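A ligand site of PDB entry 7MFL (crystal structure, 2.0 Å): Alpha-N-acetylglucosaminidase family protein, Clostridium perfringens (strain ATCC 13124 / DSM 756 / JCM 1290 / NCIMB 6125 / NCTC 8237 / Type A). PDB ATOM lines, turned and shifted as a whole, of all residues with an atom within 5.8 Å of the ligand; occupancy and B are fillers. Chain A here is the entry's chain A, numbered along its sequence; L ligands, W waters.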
ATOM      1  N   ASN A 282       3.712  28.290  -6.741  1.00  0.00           N
ATOM      2  CA  ASN A 282       4.595  27.879  -7.822  1.00  0.00           C
ATOM      3  C   ASN A 282       5.566  29.023  -8.108  1.00  0.00           C
ATOM      4  O   ASN A 282       5.260  30.183  -7.831  1.00  0.00           O
ATOM      5  CB  ASN A 282       3.752  27.572  -9.073  1.00  0.00           C
ATOM      6  CG  ASN A 282       4.499  26.766 -10.124  1.00  0.00           C
ATOM      7  OD1 ASN A 282       5.591  27.137 -10.561  1.00  0.00           O
ATOM      8  ND2 ASN A 282       3.895  25.664 -10.556  1.00  0.00           N
ATOM      9  N   CYS A 284       5.938  29.979 -10.943  1.00  0.00           N
ATOM     10  CA  CYS A 284       5.153  30.703 -11.945  1.00  0.00           C
ATOM     11  C   CYS A 284       4.205  31.715 -11.316  1.00  0.00           C
ATOM     12  O   CYS A 284       3.883  32.725 -11.949  1.00  0.00           O
ATOM     13  CB  CYS A 284       4.380  29.713 -12.814  1.00  0.00           C
ATOM     14  SG  CYS A 284       5.425  28.664 -13.863  1.00  0.00           S
ATOM     15  N   TYR A 288       2.814  35.081 -13.296  1.00  0.00           N
ATOM     16  CA  TYR A 288       1.471  35.178 -13.860  1.00  0.00           C
ATOM     17  C   TYR A 288       0.526  35.971 -12.955  1.00  0.00           C
ATOM     18  O   TYR A 288      -0.446  36.549 -13.446  1.00  0.00           O
ATOM     19  CB  TYR A 288       0.912  33.780 -14.113  1.00  0.00           C
ATOM     20  CG  TYR A 288       1.612  33.049 -15.243  1.00  0.00           C
ATOM     21  CD1 TYR A 288       1.859  33.689 -16.457  1.00  0.00           C
ATOM     22  CD2 TYR A 288       2.028  31.732 -15.098  1.00  0.00           C
ATOM     23  CE1 TYR A 288       2.498  33.020 -17.489  1.00  0.00           C
ATOM     24  CE2 TYR A 288       2.667  31.062 -16.129  1.00  0.00           C
ATOM     25  CZ  TYR A 288       2.897  31.714 -17.317  1.00  0.00           C
ATOM     26  OH  TYR A 288       3.534  31.062 -18.345  1.00  0.00           O
ATOM     27  N   TRP A 349      10.757  31.964 -14.671  1.00  0.00           N
ATOM     28  CA  TRP A 349      11.566  31.178 -15.575  1.00  0.00           C
ATOM     29  C   TRP A 349      13.029  31.595 -15.567  1.00  0.00           C
ATOM     30  O   TRP A 349      13.885  30.837 -16.039  1.00  0.00           O
ATOM     31  CB  TRP A 349      10.957  31.264 -16.966  1.00  0.00           C
ATOM     32  CG  TRP A 349       9.512  30.889 -16.873  1.00  0.00           C
ATOM     33  CD1 TRP A 349       8.994  29.629 -16.839  1.00  0.00           C
ATOM     34  CD2 TRP A 349       8.407  31.788 -16.700  1.00  0.00           C
ATOM     35  NE1 TRP A 349       7.627  29.684 -16.692  1.00  0.00           N
ATOM     36  CE2 TRP A 349       7.249  31.002 -16.606  1.00  0.00           C
ATOM     37  CE3 TRP A 349       8.292  33.186 -16.650  1.00  0.00           C
ATOM     38  CZ2 TRP A 349       5.977  31.561 -16.460  1.00  0.00           C
ATOM     39  CZ3 TRP A 349       7.028  33.734 -16.502  1.00  0.00           C
ATOM     40  CH2 TRP A 349       5.887  32.925 -16.404  1.00  0.00           C
ATOM     41  N   MET A 352      14.027  29.392 -12.446  1.00  0.00           N
ATOM     42  CA  MET A 352      14.003  27.986 -12.843  1.00  0.00           C
ATOM     43  C   MET A 352      14.983  27.698 -13.976  1.00  0.00           C
ATOM     44  O   MET A 352      14.933  26.602 -14.554  1.00  0.00           O
ATOM     45  CB  MET A 352      12.580  27.570 -13.229  1.00  0.00           C
ATOM     46  CG  MET A 352      11.630  27.565 -12.028  1.00  0.00           C
ATOM     47  SD  MET A 352      10.063  26.726 -12.311  1.00  0.00           S
ATOM     48  CE  MET A 352       9.256  27.842 -13.452  1.00  0.00           C
ATOM     49  N   ASN A 354      15.410  28.779 -17.060  1.00  0.00           N
ATOM     50  CA  ASN A 354      14.879  28.587 -18.400  1.00  0.00           C
ATOM     51  C   ASN A 354      15.186  29.729 -19.355  1.00  0.00           C
ATOM     52  O   ASN A 354      15.164  29.515 -20.576  1.00  0.00           O
ATOM     53  CB  ASN A 354      13.352  28.400 -18.351  1.00  0.00           C
ATOM     54  CG  ASN A 354      12.944  27.157 -17.582  1.00  0.00           C
ATOM     55  OD1 ASN A 354      11.977  27.181 -16.813  1.00  0.00           O
ATOM     56  ND2 ASN A 354      13.666  26.069 -17.782  1.00  0.00           N
ATOM     57  N   TRP A 416      15.192  26.825 -24.276  1.00  0.00           N
ATOM     58  CA  TRP A 416      13.876  26.596 -23.676  1.00  0.00           C
ATOM     59  C   TRP A 416      12.901  27.543 -24.360  1.00  0.00           C
ATOM     60  O   TRP A 416      12.993  28.755 -24.171  1.00  0.00           O
ATOM     61  CB  TRP A 416      13.903  26.825 -22.164  1.00  0.00           C
ATOM     62  CG  TRP A 416      12.571  26.644 -21.484  1.00  0.00           C
ATOM     63  CD1 TRP A 416      12.054  25.483 -20.984  1.00  0.00           C
ATOM     64  CD2 TRP A 416      11.599  27.656 -21.231  1.00  0.00           C
ATOM     65  NE1 TRP A 416      10.818  25.719 -20.439  1.00  0.00           N
ATOM     66  CE2 TRP A 416      10.515  27.042 -20.572  1.00  0.00           C
ATOM     67  CE3 TRP A 416      11.530  29.038 -21.491  1.00  0.00           C
ATOM     68  CZ2 TRP A 416       9.377  27.746 -20.181  1.00  0.00           C
ATOM     69  CZ3 TRP A 416      10.401  29.731 -21.097  1.00  0.00           C
ATOM     70  CH2 TRP A 416       9.335  29.091 -20.451  1.00  0.00           C
ATOM     71  N   CYS A 417      11.999  26.987 -25.159  1.00  0.00           N
ATOM     72  CA  CYS A 417      10.972  27.766 -25.870  1.00  0.00           C
ATOM     73  C   CYS A 417      11.589  28.922 -26.642  1.00  0.00           C
ATOM     74  O   CYS A 417      11.060  30.040 -26.655  1.00  0.00           O
ATOM     75  CB  CYS A 417       9.900  28.265 -24.901  1.00  0.00           C
ATOM     76  SG  CYS A 417       8.995  26.969 -24.040  1.00  0.00           S
ATOM     77  N   HIS A 465      15.207  21.808 -14.981  1.00  0.00           N
ATOM     78  CA  HIS A 465      13.770  21.998 -15.021  1.00  0.00           C
ATOM     79  C   HIS A 465      13.301  22.132 -16.474  1.00  0.00           C
ATOM     80  O   HIS A 465      13.678  23.093 -17.159  1.00  0.00           O
ATOM     81  CB  HIS A 465      13.359  23.225 -14.218  1.00  0.00           C
ATOM     82  CG  HIS A 465      11.878  23.460 -14.180  1.00  0.00           C
ATOM     83  ND1 HIS A 465      11.021  22.690 -13.437  1.00  0.00           N
ATOM     84  CD2 HIS A 465      11.109  24.384 -14.800  1.00  0.00           C
ATOM     85  CE1 HIS A 465       9.784  23.129 -13.593  1.00  0.00           C
ATOM     86  NE2 HIS A 465       9.812  24.153 -14.421  1.00  0.00           N
ATOM     87  N   GLU A 466      12.520  21.161 -16.931  1.00  0.00           N
ATOM     88  CA  GLU A 466      11.948  21.150 -18.282  1.00  0.00           C
ATOM     89  C   GLU A 466      13.018  21.177 -19.366  1.00  0.00           C
ATOM     90  O   GLU A 466      12.816  21.754 -20.444  1.00  0.00           O
ATOM     91  CB  GLU A 466      10.960  22.313 -18.478  1.00  0.00           C
ATOM     92  CG  GLU A 466       9.659  22.144 -17.716  1.00  0.00           C
ATOM     93  CD  GLU A 466       8.534  22.982 -18.301  1.00  0.00           C
ATOM     94  OE1 GLU A 466       8.813  24.095 -18.792  1.00  0.00           O
ATOM     95  OE2 GLU A 466       7.372  22.527 -18.266  1.00  0.00           O
ATOM     96  N   GLN A 498      10.970  20.351  -6.725  1.00  0.00           N
ATOM     97  CA  GLN A 498       9.780  20.141  -7.534  1.00  0.00           C
ATOM     98  C   GLN A 498       9.829  18.780  -8.207  1.00  0.00           C
ATOM     99  O   GLN A 498      10.885  18.332  -8.658  1.00  0.00           O
ATOM    100  CB  GLN A 498       9.666  21.217  -8.618  1.00  0.00           C
ATOM    101  CG  GLN A 498       9.469  22.641  -8.115  1.00  0.00           C
ATOM    102  CD  GLN A 498       9.229  23.601  -9.267  1.00  0.00           C
ATOM    103  OE1 GLN A 498       8.141  23.646  -9.830  1.00  0.00           O
ATOM    104  NE2 GLN A 498      10.259  24.369  -9.618  1.00  0.00           N
ATOM    105  N   TRP A 500       8.065  17.307 -11.387  1.00  0.00           N
ATOM    106  CA  TRP A 500       7.288  17.720 -12.555  1.00  0.00           C
ATOM    107  C   TRP A 500       7.617  16.816 -13.725  1.00  0.00           C
ATOM    108  O   TRP A 500       8.785  16.676 -14.107  1.00  0.00           O
ATOM    109  CB  TRP A 500       7.571  19.184 -12.897  1.00  0.00           C
ATOM    110  CG  TRP A 500       6.892  19.700 -14.137  1.00  0.00           C
ATOM    111  CD1 TRP A 500       7.491  20.259 -15.229  1.00  0.00           C
ATOM    112  CD2 TRP A 500       5.478  19.723 -14.397  1.00  0.00           C
ATOM    113  NE1 TRP A 500       6.551  20.617 -16.155  1.00  0.00           N
ATOM    114  CE2 TRP A 500       5.308  20.296 -15.671  1.00  0.00           C
ATOM    115  CE3 TRP A 500       4.355  19.312 -13.683  1.00  0.00           C
ATOM    116  CZ2 TRP A 500       4.050  20.470 -16.246  1.00  0.00           C
ATOM    117  CZ3 TRP A 500       3.103  19.492 -14.253  1.00  0.00           C
ATOM    118  CH2 TRP A 500       2.961  20.060 -15.518  1.00  0.00           C
ATOM    119  N   LEU A 523       3.922  17.960  -7.768  1.00  0.00           N
ATOM    120  CA  LEU A 523       3.377  19.229  -8.230  1.00  0.00           C
ATOM    121  C   LEU A 523       1.946  19.131  -8.731  1.00  0.00           C
ATOM    122  O   LEU A 523       1.214  20.122  -8.676  1.00  0.00           O
ATOM    123  CB  LEU A 523       4.266  19.812  -9.330  1.00  0.00           C
ATOM    124  CG  LEU A 523       4.489  21.315  -9.278  1.00  0.00           C
ATOM    125  CD1 LEU A 523       5.393  21.687  -8.108  1.00  0.00           C
ATOM    126  CD2 LEU A 523       5.069  21.826 -10.592  1.00  0.00           C
ATOM    127  N   LEU A 546      -2.232  21.565  -8.332  1.00  0.00           N
ATOM    128  CA  LEU A 546      -1.750  22.585  -9.252  1.00  0.00           C
ATOM    129  C   LEU A 546      -2.912  23.422  -9.793  1.00  0.00           C
ATOM    130  O   LEU A 546      -2.942  24.640  -9.617  1.00  0.00           O
ATOM    131  CB  LEU A 546      -0.971  21.926 -10.398  1.00  0.00           C
ATOM    132  CG  LEU A 546       0.206  22.693 -10.990  1.00  0.00           C
ATOM    133  CD1 LEU A 546       1.139  21.744 -11.740  1.00  0.00           C
ATOM    134  CD2 LEU A 546      -0.269  23.801 -11.916  1.00  0.00           C
ATOM    135  N   PHE A 549      -3.060  26.772 -14.768  1.00  0.00           N
ATOM    136  CA  PHE A 549      -1.943  26.888 -15.704  1.00  0.00           C
ATOM    137  C   PHE A 549      -2.009  28.245 -16.381  1.00  0.00           C
ATOM    138  O   PHE A 549      -3.026  28.577 -17.010  1.00  0.00           O
ATOM    139  CB  PHE A 549      -1.967  25.768 -16.744  1.00  0.00           C
ATOM    140  CG  PHE A 549      -1.475  24.435 -16.230  1.00  0.00           C
ATOM    141  CD1 PHE A 549      -0.172  24.032 -16.460  1.00  0.00           C
ATOM    142  CD2 PHE A 549      -2.323  23.602 -15.524  1.00  0.00           C
ATOM    143  CE1 PHE A 549       0.280  22.814 -15.982  1.00  0.00           C
ATOM    144  CE2 PHE A 549      -1.877  22.378 -15.051  1.00  0.00           C
ATOM    145  CZ  PHE A 549      -0.575  21.983 -15.289  1.00  0.00           C
ATOM    146  N   THR A 582       0.135  24.526  -5.809  1.00  0.00           N
ATOM    147  CA  THR A 582       1.235  24.897  -6.695  1.00  0.00           C
ATOM    148  C   THR A 582       0.711  25.574  -7.966  1.00  0.00           C
ATOM    149  O   THR A 582       1.187  25.253  -9.058  1.00  0.00           O
ATOM    150  CB  THR A 582       2.045  23.663  -7.068  1.00  0.00           C
ATOM    151  OG1 THR A 582       1.149  22.605  -7.450  1.00  0.00           O
ATOM    152  CG2 THR A 582       2.892  23.203  -5.895  1.00  0.00           C
ATOM    153  N   GLU A 584       0.093  27.967 -11.130  1.00  0.00           N
ATOM    154  CA  GLU A 584       0.867  28.921 -11.893  1.00  0.00           C
ATOM    155  C   GLU A 584       0.300  30.328 -11.774  1.00  0.00           C
ATOM    156  O   GLU A 584       0.998  31.303 -12.089  1.00  0.00           O
ATOM    157  CB  GLU A 584       0.962  28.472 -13.353  1.00  0.00           C
ATOM    158  CG  GLU A 584       1.665  27.133 -13.496  1.00  0.00           C
ATOM    159  CD  GLU A 584       1.863  26.710 -14.936  1.00  0.00           C
ATOM    160  OE1 GLU A 584       1.389  27.420 -15.858  1.00  0.00           O
ATOM    161  OE2 GLU A 584       2.495  25.660 -15.148  1.00  0.00           O
ATOM    162  N   GLN A 647      -4.162  20.097 -18.694  1.00  0.00           N
ATOM    163  CA  GLN A 647      -3.455  21.200 -18.050  1.00  0.00           C
ATOM    164  C   GLN A 647      -4.382  22.418 -18.005  1.00  0.00           C
ATOM    165  O   GLN A 647      -4.474  23.177 -18.972  1.00  0.00           O
ATOM    166  CB  GLN A 647      -2.157  21.523 -18.782  1.00  0.00           C
ATOM    167  CG  GLN A 647      -1.107  20.422 -18.684  1.00  0.00           C
ATOM    168  CD  GLN A 647       0.288  20.914 -19.042  1.00  0.00           C
ATOM    169  OE1 GLN A 647       0.484  22.073 -19.393  1.00  0.00           O
ATOM    170  NE2 GLN A 647       1.260  20.009 -18.966  1.00  0.00           N
ATOM    171  N   TRP A 668       0.005  23.575 -25.062  1.00  0.00           N
ATOM    172  CA  TRP A 668      -0.207  22.402 -24.219  1.00  0.00           C
ATOM    173  C   TRP A 668      -1.569  22.422 -23.529  1.00  0.00           C
ATOM    174  O   TRP A 668      -1.773  21.697 -22.551  1.00  0.00           O
ATOM    175  CB  TRP A 668       0.916  22.276 -23.192  1.00  0.00           C
ATOM    176  CG  TRP A 668       2.262  22.322 -23.840  1.00  0.00           C
ATOM    177  CD1 TRP A 668       2.959  21.285 -24.377  1.00  0.00           C
ATOM    178  CD2 TRP A 668       3.062  23.490 -24.047  1.00  0.00           C
ATOM    179  NE1 TRP A 668       4.154  21.725 -24.893  1.00  0.00           N
ATOM    180  CE2 TRP A 668       4.238  23.073 -24.705  1.00  0.00           C
ATOM    181  CE3 TRP A 668       2.917  24.852 -23.743  1.00  0.00           C
ATOM    182  CZ2 TRP A 668       5.254  23.963 -25.057  1.00  0.00           C
ATOM    183  CZ3 TRP A 668       3.928  25.730 -24.093  1.00  0.00           C
ATOM    184  CH2 TRP A 668       5.079  25.278 -24.742  1.00  0.00           C
ATOM    185  N   TRP A 794       3.927  36.309 -24.934  1.00  0.00           N
ATOM    186  CA  TRP A 794       4.855  35.769 -23.937  1.00  0.00           C
ATOM    187  C   TRP A 794       6.264  36.291 -24.193  1.00  0.00           C
ATOM    188  O   TRP A 794       6.793  37.070 -23.398  1.00  0.00           O
ATOM    189  CB  TRP A 794       4.832  34.237 -23.930  1.00  0.00           C
ATOM    190  CG  TRP A 794       5.060  33.622 -22.589  1.00  0.00           C
ATOM    191  CD1 TRP A 794       4.120  33.054 -21.775  1.00  0.00           C
ATOM    192  CD2 TRP A 794       6.311  33.470 -21.918  1.00  0.00           C
ATOM    193  NE1 TRP A 794       4.713  32.581 -20.628  1.00  0.00           N
ATOM    194  CE2 TRP A 794       6.065  32.822 -20.696  1.00  0.00           C
ATOM    195  CE3 TRP A 794       7.633  33.830 -22.221  1.00  0.00           C
ATOM    196  CZ2 TRP A 794       7.064  32.514 -19.780  1.00  0.00           C
ATOM    197  CZ3 TRP A 794       8.631  33.537 -21.318  1.00  0.00           C
ATOM    198  CH2 TRP A 794       8.344  32.882 -20.116  1.00  0.00           C
ATOM    199  N   LEU A 805       5.029  29.397 -27.138  1.00  0.00           N
ATOM    200  CA  LEU A 805       4.480  30.108 -25.995  1.00  0.00           C
ATOM    201  C   LEU A 805       3.327  31.040 -26.350  1.00  0.00           C
ATOM    202  O   LEU A 805       2.787  31.704 -25.446  1.00  0.00           O
ATOM    203  CB  LEU A 805       5.580  30.922 -25.302  1.00  0.00           C
ATOM    204  CG  LEU A 805       6.602  30.089 -24.532  1.00  0.00           C
ATOM    205  CD1 LEU A 805       7.751  30.958 -24.059  1.00  0.00           C
ATOM    206  CD2 LEU A 805       5.931  29.391 -23.378  1.00  0.00           C
ATOM    207  N   TYR A 808       0.028  31.502 -24.232  1.00  0.00           N
ATOM    208  CA  TYR A 808       0.063  30.550 -23.130  1.00  0.00           C
ATOM    209  C   TYR A 808      -0.717  31.075 -21.936  1.00  0.00           C
ATOM    210  O   TYR A 808      -1.437  30.320 -21.274  1.00  0.00           O
ATOM    211  CB  TYR A 808       1.509  30.234 -22.715  1.00  0.00           C
ATOM    212  CG  TYR A 808       1.550  29.271 -21.552  1.00  0.00           C
ATOM    213  CD1 TYR A 808       1.619  27.898 -21.761  1.00  0.00           C
ATOM    214  CD2 TYR A 808       1.489  29.735 -20.237  1.00  0.00           C
ATOM    215  CE1 TYR A 808       1.634  27.022 -20.694  1.00  0.00           C
ATOM    216  CE2 TYR A 808       1.503  28.865 -19.177  1.00  0.00           C
ATOM    217  CZ  TYR A 808       1.578  27.520 -19.401  1.00  0.00           C
ATOM    218  OH  TYR A 808       1.590  26.660 -18.331  1.00  0.00           O
HETATM  219  C1  LIG L   1       5.446  28.317 -20.037  1.00  0.00           C
HETATM  220  C2  LIG L   1       5.032  23.221 -13.926  1.00  0.00           C
HETATM  221  C3  LIG L   1       3.346  24.253 -18.357  1.00  0.00           C
HETATM  222  C4  LIG L   1       5.152  27.765 -18.639  1.00  0.00           C
HETATM  223  C5  LIG L   1       5.402  23.788 -15.297  1.00  0.00           C
HETATM  224  C6  LIG L   1       4.567  24.335 -17.453  1.00  0.00           C
HETATM  225  C7  LIG L   1       5.841  25.185 -15.052  1.00  0.00           C
HETATM  226  C8  LIG L   1       6.163  25.841 -16.387  1.00  0.00           C
HETATM  227  C9  LIG L   1       4.879  25.801 -17.243  1.00  0.00           C
HETATM  228  N1  LIG L   1       5.146  26.423 -18.536  1.00  0.00           N
HETATM  229  N2  LIG L   1       4.230  23.704 -16.163  1.00  0.00           N
HETATM  230  O1  LIG L   1       4.803  28.517 -17.729  1.00  0.00           O
HETATM  231  O2  LIG L   1       3.983  24.022 -13.367  1.00  0.00           O
HETATM  232  O3  LIG L   1       3.018  22.878 -18.586  1.00  0.00           O
HETATM  233  O4  LIG L   1       7.032  25.134 -14.271  1.00  0.00           O
HETATM  234  O5  LIG L   1       6.690  27.169 -16.191  1.00  0.00           O
HETATM  235  O   HOH W   1       9.610  26.078 -16.900  1.00  0.00           O
HETATM  236  O   HOH W   2       3.783  20.193 -20.532  1.00  0.00           O
HETATM  237  O   HOH W   3       6.947  25.106 -11.818  1.00  0.00           O
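The indole nitrogen of Trp 349 sits at hydrogen-bond distance from an oxygen (O5) of the ligand (2.7 Å).
The side-chain amide oxygen (OE1) of Gln 647 lies within hydrogen-bond range of an oxygen (O3) of the ligand, 2.8 Å away.
The side-chain carboxylate (OE2) of Glu 584 lies within salt-bridge range of a nitrogen (N2) of the ligand (2.8 Å).
The side-chain hydroxyl (OH) of Tyr 288 lies within hydrogen-bond range of an oxygen (O1) of the ligand, at 2.9 Å.
NE2 of His 465 lies within hydrogen-bond range of O4 of the ligand.
An oxygen (O5) of the ligand sits at hydrogen-bond distance from the side-chain sulfur (SG) of Cys 284 (3.0 Å).
ND2 of Asn 282 sits at hydrogen-bond distance from O2 of the ligand (3.3 Å).
A nitrogen (N2) of the ligand is in salt-bridge range of the side-chain carboxylate of Glu 466 (3.96 Å).
NE1 of Trp 349 lies within hydrogen-bond range of SG of Cys 284, 3.7 Å away.
N of Asn 354 lies within hydrogen-bond range of O of Trp 349 (2.8 Å).
OH of Tyr 808 lies within hydrogen-bond range of OE1 of Glu 584 (2.6 Å).
The indole nitrogen (NE1) of Trp 794 is in hydrogen-bond range of the side-chain hydroxyl (OH) of Tyr 288 (3.0 Å).
The backbone carbonyl oxygen of His 465 sits at hydrogen-bond distance from the side-chain amide nitrogen of Asn 354 (3.0 Å).
O of Thr 582 is in hydrogen-bond range of ND2 of Asn 282, at 3.1 Å.
NE2 of Gln 498 is in hydrogen-bond range of SD of Met 352, 3.6 Å away.
The backbone carbonyl oxygen (O) of Leu 523 is in hydrogen-bond range of the side-chain hydroxyl (OG1) of Thr 582 (2.8 Å).
Met 352 touches the ligand.
CZ2 of Trp 416 touches C1 of the ligand, 3.97 Å away.
CZ2 of Trp 500 touches N2 of the ligand (3.2 Å).
Leu 523 touches the ligand.
CD1 of Leu 546 touches O2 of the ligand, at 3.99 Å.
Phe 549 touches the ligand (CE1 to O3, 3.8 Å).
Leu 805 touches the ligand.
Tyr 808 touches the ligand (OH to C3, 3.0 Å).
Hydrophobic or aromatic side chains within 4 Å of the ligand: Tyr 288, Trp 349, Met 352, Trp 416, His 465, Trp 500, Leu 523, Leu 546, Phe 549, Leu 805 and Tyr 808.
Within 4 Å of the ligand: Asn 282, Cys 284, Tyr 288, Trp 349, Met 352, Trp 416, His 465, Glu 466, Trp 500, Leu 523, Leu 546, Phe 549, Glu 584, Gln 647, Leu 805 and Tyr 808.
Water W1 lies within hydrogen-bond range of OD1 of Asn 354, OE1 of Glu 466, NE2 of His 465 and O5 of the ligand.
Water W2 lies within hydrogen-bond range of the side-chain amide nitrogen of Gln 647 and an oxygen (O3) of the ligand.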
